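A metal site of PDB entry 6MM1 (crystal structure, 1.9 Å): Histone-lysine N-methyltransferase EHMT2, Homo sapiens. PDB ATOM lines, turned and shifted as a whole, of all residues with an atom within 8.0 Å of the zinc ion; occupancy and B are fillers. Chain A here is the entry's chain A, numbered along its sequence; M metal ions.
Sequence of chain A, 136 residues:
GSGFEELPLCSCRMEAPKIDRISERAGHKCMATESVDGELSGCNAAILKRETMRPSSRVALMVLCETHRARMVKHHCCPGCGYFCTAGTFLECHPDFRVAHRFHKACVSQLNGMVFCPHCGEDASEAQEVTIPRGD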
ATOM      1  N   LYS A  29       4.090   9.467  25.518  1.00  0.00           N
ATOM      2  CA  LYS A  29       3.508   8.723  26.621  1.00  0.00           C
ATOM      3  C   LYS A  29       1.996   8.876  26.601  1.00  0.00           C
ATOM      4  O   LYS A  29       1.468   9.954  26.301  1.00  0.00           O
ATOM      5  CB  LYS A  29       4.070   9.209  27.957  1.00  0.00           C
ATOM      6  CG  LYS A  29       5.591   9.215  28.033  1.00  0.00           C
ATOM      7  CD  LYS A  29       6.084   9.656  29.411  1.00  0.00           C
ATOM      8  CE  LYS A  29       7.276  10.588  29.297  1.00  0.00           C
ATOM      9  NZ  LYS A  29       8.311  10.034  28.373  1.00  0.00           N
ATOM     10  N   CYS A  30       1.299   7.794  26.949  1.00  0.00           N
ATOM     11  CA  CYS A  30      -0.150   7.771  26.842  1.00  0.00           C
ATOM     12  C   CYS A  30      -0.786   8.858  27.690  1.00  0.00           C
ATOM     13  O   CYS A  30      -0.418   9.059  28.858  1.00  0.00           O
ATOM     14  CB  CYS A  30      -0.666   6.398  27.248  1.00  0.00           C
ATOM     15  SG  CYS A  30      -2.444   6.219  27.214  1.00  0.00           S
ATOM     16  N   MET A  31      -1.755   9.571  27.112  1.00  0.00           N
ATOM     17  CA  MET A  31      -2.432  10.676  27.768  1.00  0.00           C
ATOM     18  C   MET A  31      -3.758  10.270  28.420  1.00  0.00           C
ATOM     19  O   MET A  31      -4.518  11.150  28.833  1.00  0.00           O
ATOM     20  CB  MET A  31      -2.692  11.803  26.755  1.00  0.00           C
ATOM     21  CG  MET A  31      -1.424  12.512  26.297  1.00  0.00           C
ATOM     22  SD  MET A  31      -1.624  13.553  24.822  1.00  0.00           S
ATOM     23  CE  MET A  31      -2.851  14.730  25.393  1.00  0.00           C
ATOM     24  N   ALA A  32      -4.040   8.971  28.545  1.00  0.00           N
ATOM     25  CA  ALA A  32      -5.314   8.530  29.100  1.00  0.00           C
ATOM     26  C   ALA A  32      -5.427   8.861  30.583  1.00  0.00           C
ATOM     27  O   ALA A  32      -4.445   8.853  31.325  1.00  0.00           O
ATOM     28  CB  ALA A  32      -5.474   7.019  28.901  1.00  0.00           C
ATOM     29  N   THR A  33      -6.652   9.145  31.007  1.00  0.00           N
ATOM     30  CA  THR A  33      -6.987   9.290  32.418  1.00  0.00           C
ATOM     31  C   THR A  33      -8.031   8.254  32.803  1.00  0.00           C
ATOM     32  O   THR A  33      -9.131   8.240  32.232  1.00  0.00           O
ATOM     33  CB  THR A  33      -7.506  10.688  32.713  1.00  0.00           C
ATOM     34  OG1 THR A  33      -6.541  11.641  32.299  1.00  0.00           O
ATOM     35  CG2 THR A  33      -7.782  10.864  34.189  1.00  0.00           C
ATOM     36  N   GLU A  34      -7.697   7.388  33.762  1.00  0.00           N
ATOM     37  CA  GLU A  34      -8.645   6.431  34.312  1.00  0.00           C
ATOM     38  C   GLU A  34      -9.427   7.047  35.464  1.00  0.00           C
ATOM     39  O   GLU A  34      -8.876   7.780  36.289  1.00  0.00           O
ATOM     40  CB  GLU A  34      -7.915   5.174  34.800  1.00  0.00           C
ATOM     41  CG  GLU A  34      -7.320   4.329  33.701  1.00  0.00           C
ATOM     42  CD  GLU A  34      -8.366   3.479  32.985  1.00  0.00           C
ATOM     43  OE1 GLU A  34      -9.519   3.401  33.480  1.00  0.00           O
ATOM     44  OE2 GLU A  34      -8.018   2.888  31.941  1.00  0.00           O
ATOM     45  N   GLY A  42      -3.341   8.389  36.038  1.00  0.00           N
ATOM     46  CA  GLY A  42      -2.799   8.521  34.699  1.00  0.00           C
ATOM     47  C   GLY A  42      -2.330   7.202  34.134  1.00  0.00           C
ATOM     48  O   GLY A  42      -2.429   6.143  34.760  1.00  0.00           O
ATOM     49  N   CYS A  43      -1.821   7.258  32.903  1.00  0.00           N
ATOM     50  CA  CYS A  43      -1.221   6.093  32.272  1.00  0.00           C
ATOM     51  C   CYS A  43       0.253   6.347  32.010  1.00  0.00           C
ATOM     52  O   CYS A  43       1.115   5.830  32.731  1.00  0.00           O
ATOM     53  CB  CYS A  43      -1.934   5.727  30.977  1.00  0.00           C
ATOM     54  SG  CYS A  43      -1.251   4.242  30.165  1.00  0.00           S
ATOM     55  N   ASN A  44       0.546   7.132  30.972  1.00  0.00           N
ATOM     56  CA  ASN A  44       1.913   7.499  30.554  1.00  0.00           C
ATOM     57  C   ASN A  44       2.748   6.299  30.101  1.00  0.00           C
ATOM     58  O   ASN A  44       3.983   6.382  30.073  1.00  0.00           O
ATOM     59  CB  ASN A  44       2.637   8.275  31.661  1.00  0.00           C
ATOM     60  CG  ASN A  44       1.893   9.542  32.072  1.00  0.00           C
ATOM     61  OD1 ASN A  44       1.645  10.429  31.248  1.00  0.00           O
ATOM     62  ND2 ASN A  44       1.529   9.624  33.339  1.00  0.00           N
ATOM     63  N   ALA A  45       2.114   5.201  29.717  1.00  0.00           N
ATOM     64  CA  ALA A  45       2.811   4.129  29.030  1.00  0.00           C
ATOM     65  C   ALA A  45       3.281   4.594  27.641  1.00  0.00           C
ATOM     66  O   ALA A  45       2.713   5.509  27.043  1.00  0.00           O
ATOM     67  CB  ALA A  45       1.931   2.890  28.877  1.00  0.00           C
ATOM     68  N   ALA A  46       4.308   3.930  27.141  1.00  0.00           N
ATOM     69  CA  ALA A  46       4.875   4.296  25.856  1.00  0.00           C
ATOM     70  C   ALA A  46       3.891   3.974  24.738  1.00  0.00           C
ATOM     71  O   ALA A  46       3.246   2.920  24.742  1.00  0.00           O
ATOM     72  CB  ALA A  46       6.183   3.557  25.613  1.00  0.00           C
ATOM     73  N   ILE A  47       3.772   4.903  23.788  1.00  0.00           N
ATOM     74  CA  ILE A  47       2.783   4.805  22.724  1.00  0.00           C
ATOM     75  C   ILE A  47       3.446   4.241  21.466  1.00  0.00           C
ATOM     76  O   ILE A  47       4.658   4.379  21.257  1.00  0.00           O
ATOM     77  CB  ILE A  47       2.140   6.180  22.447  1.00  0.00           C
ATOM     78  CG1 ILE A  47       3.182   7.174  21.968  1.00  0.00           C
ATOM     79  CG2 ILE A  47       1.530   6.744  23.725  1.00  0.00           C
ATOM     80  CD1 ILE A  47       3.094   7.474  20.496  1.00  0.00           C
ATOM     81  N   VAL A  63      -3.036  11.283  22.430  1.00  0.00           N
ATOM     82  CA  VAL A  63      -2.292  10.120  21.978  1.00  0.00           C
ATOM     83  C   VAL A  63      -2.417   9.034  23.051  1.00  0.00           C
ATOM     84  O   VAL A  63      -2.425   9.337  24.259  1.00  0.00           O
ATOM     85  CB  VAL A  63      -0.822  10.483  21.667  1.00  0.00           C
ATOM     86  CG1 VAL A  63      -0.078  10.921  22.922  1.00  0.00           C
ATOM     87  CG2 VAL A  63      -0.093   9.341  20.995  1.00  0.00           C
ATOM     88  N   LEU A  64      -2.557   7.781  22.640  1.00  0.00           N
ATOM     89  CA  LEU A  64      -2.856   6.694  23.553  1.00  0.00           C
ATOM     90  C   LEU A  64      -1.968   5.501  23.301  1.00  0.00           C
ATOM     91  O   LEU A  64      -1.612   5.202  22.156  1.00  0.00           O
ATOM     92  CB  LEU A  64      -4.310   6.229  23.421  1.00  0.00           C
ATOM     93  CG  LEU A  64      -5.369   7.283  23.708  1.00  0.00           C
ATOM     94  CD1 LEU A  64      -6.725   6.799  23.255  1.00  0.00           C
ATOM     95  CD2 LEU A  64      -5.366   7.616  25.185  1.00  0.00           C
ATOM     96  N   CYS A  65      -1.666   4.775  24.385  1.00  0.00           N
ATOM     97  CA  CYS A  65      -1.018   3.478  24.289  1.00  0.00           C
ATOM     98  C   CYS A  65      -1.979   2.464  23.670  1.00  0.00           C
ATOM     99  O   CYS A  65      -3.181   2.691  23.553  1.00  0.00           O
ATOM    100  CB  CYS A  65      -0.548   3.000  25.669  1.00  0.00           C
ATOM    101  SG  CYS A  65      -1.860   2.423  26.825  1.00  0.00           S
ATOM    102  N   GLU A  66      -1.438   1.324  23.256  1.00  0.00           N
ATOM    103  CA  GLU A  66      -2.270   0.375  22.514  1.00  0.00           C
ATOM    104  C   GLU A  66      -3.412  -0.153  23.361  1.00  0.00           C
ATOM    105  O   GLU A  66      -4.515  -0.386  22.839  1.00  0.00           O
ATOM    106  CB  GLU A  66      -1.409  -0.768  21.973  1.00  0.00           C
ATOM    107  CG  GLU A  66      -0.555  -0.366  20.769  1.00  0.00           C
ATOM    108  CD  GLU A  66      -1.375   0.247  19.637  1.00  0.00           C
ATOM    109  OE1 GLU A  66      -1.323   1.489  19.460  1.00  0.00           O
ATOM    110  OE2 GLU A  66      -2.088  -0.512  18.941  1.00  0.00           O
ATOM    111  N   THR A  67      -3.193  -0.332  24.663  1.00  0.00           N
ATOM    112  CA  THR A  67      -4.254  -0.792  25.556  1.00  0.00           C
ATOM    113  C   THR A  67      -5.391   0.216  25.646  1.00  0.00           C
ATOM    114  O   THR A  67      -6.571  -0.152  25.630  1.00  0.00           O
ATOM    115  CB  THR A  67      -3.682  -1.070  26.947  1.00  0.00           C
ATOM    116  OG1 THR A  67      -2.745  -2.152  26.884  1.00  0.00           O
ATOM    117  CG2 THR A  67      -4.791  -1.427  27.923  1.00  0.00           C
ATOM    118  N   HIS A  68      -5.053   1.501  25.732  1.00  0.00           N
ATOM    119  CA  HIS A  68      -6.098   2.492  25.860  1.00  0.00           C
ATOM    120  C   HIS A  68      -6.760   2.812  24.529  1.00  0.00           C
ATOM    121  O   HIS A  68      -7.937   3.196  24.524  1.00  0.00           O
ATOM    122  CB  HIS A  68      -5.543   3.749  26.534  1.00  0.00           C
ATOM    123  CG  HIS A  68      -5.570   3.662  28.030  1.00  0.00           C
ATOM    124  ND1 HIS A  68      -4.424   3.630  28.799  1.00  0.00           N
ATOM    125  CD2 HIS A  68      -6.606   3.561  28.895  1.00  0.00           C
ATOM    126  CE1 HIS A  68      -4.759   3.515  30.069  1.00  0.00           C
ATOM    127  NE2 HIS A  68      -6.070   3.474  30.161  1.00  0.00           N
ATOM    128  N   ARG A  69      -6.057   2.662  23.405  1.00  0.00           N
ATOM    129  CA  ARG A  69      -6.750   2.720  22.113  1.00  0.00           C
ATOM    130  C   ARG A  69      -7.731   1.561  21.970  1.00  0.00           C
ATOM    131  O   ARG A  69      -8.852   1.738  21.454  1.00  0.00           O
ATOM    132  CB  ARG A  69      -5.740   2.682  20.958  1.00  0.00           C
ATOM    133  CG  ARG A  69      -4.827   3.883  20.901  1.00  0.00           C
ATOM    134  CD  ARG A  69      -3.728   3.686  19.869  1.00  0.00           C
ATOM    135  NE  ARG A  69      -4.298   3.453  18.553  1.00  0.00           N
ATOM    136  CZ  ARG A  69      -4.510   4.413  17.672  1.00  0.00           C
ATOM    137  NH1 ARG A  69      -4.207   5.679  17.972  1.00  0.00           N
ATOM    138  NH2 ARG A  69      -5.032   4.121  16.490  1.00  0.00           N
ATOM    139  N   ARG A  71      -9.290   0.091  24.403  1.00  0.00           N
ATOM    140  CA  ARG A  71     -10.460   0.361  25.243  1.00  0.00           C
ATOM    141  C   ARG A  71     -11.309   1.481  24.648  1.00  0.00           C
ATOM    142  O   ARG A  71     -12.541   1.451  24.709  1.00  0.00           O
ATOM    143  CB  ARG A  71     -10.023   0.674  26.670  1.00  0.00           C
ATOM    144  CG  ARG A  71      -9.425  -0.526  27.390  1.00  0.00           C
ATOM    145  CD  ARG A  71      -8.912  -0.148  28.755  1.00  0.00           C
ATOM    146  NE  ARG A  71      -8.234  -1.274  29.403  1.00  0.00           N
ATOM    147  CZ  ARG A  71      -7.374  -1.143  30.410  1.00  0.00           C
ATOM    148  NH1 ARG A  71      -7.104   0.063  30.895  1.00  0.00           N
ATOM    149  NH2 ARG A  71      -6.799  -2.216  30.927  1.00  0.00           N
ATOM    150  N   PHE A  84     -11.631   7.182  31.225  1.00  0.00           N
ATOM    151  CA  PHE A  84     -11.918   5.781  30.962  1.00  0.00           C
ATOM    152  C   PHE A  84     -12.668   5.158  32.131  1.00  0.00           C
ATOM    153  O   PHE A  84     -12.352   5.410  33.298  1.00  0.00           O
ATOM    154  CB  PHE A  84     -10.633   5.010  30.700  1.00  0.00           C
ATOM    155  CG  PHE A  84     -10.110   5.193  29.311  1.00  0.00           C
ATOM    156  CD1 PHE A  84      -9.339   6.287  28.992  1.00  0.00           C
ATOM    157  CD2 PHE A  84     -10.401   4.254  28.319  1.00  0.00           C
ATOM    158  CE1 PHE A  84      -8.848   6.451  27.707  1.00  0.00           C
ATOM    159  CE2 PHE A  84      -9.918   4.413  27.037  1.00  0.00           C
ATOM    160  CZ  PHE A  84      -9.137   5.515  26.729  1.00  0.00           C
HETATM  161 ZN    ZN M   1      -2.523   4.092  28.204  1.00  0.00          ZN
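A ring nitrogen (NE2) of His 68 lies within hydrogen-bond range of the side-chain carboxylate (OE2) of Glu 34, 2.7 Å away. The side-chain sulfur of Cys 65 lies close to the backbone NH of Thr 67, 3.7 Å away. N of Cys 43 is in hydrogen-bond range of O of Ala 32. The side-chain sulfur of Cys 43 lies close to the backbone NH of Ala 45, at 3.5 Å. N of Ala 32 sits close to SG of Cys 30 (3.4 Å). The backbone NH (N) of Cys 30 sits at hydrogen-bond distance from the backbone carbonyl oxygen (O) of Ala 45 (2.7 Å). O of Cys 30 lies within hydrogen-bond range of N of Asn 44 (3.0 Å).
Within 4 Å of the zinc ion: Cys 30, Cys 43, Cys 65 and His 68.
The zinc ion is bound by ND1 of His 68, SG of Cys 65, SG of Cys 43 and SG of Cys 30. The zinc ion has four donor atoms within binding distance.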
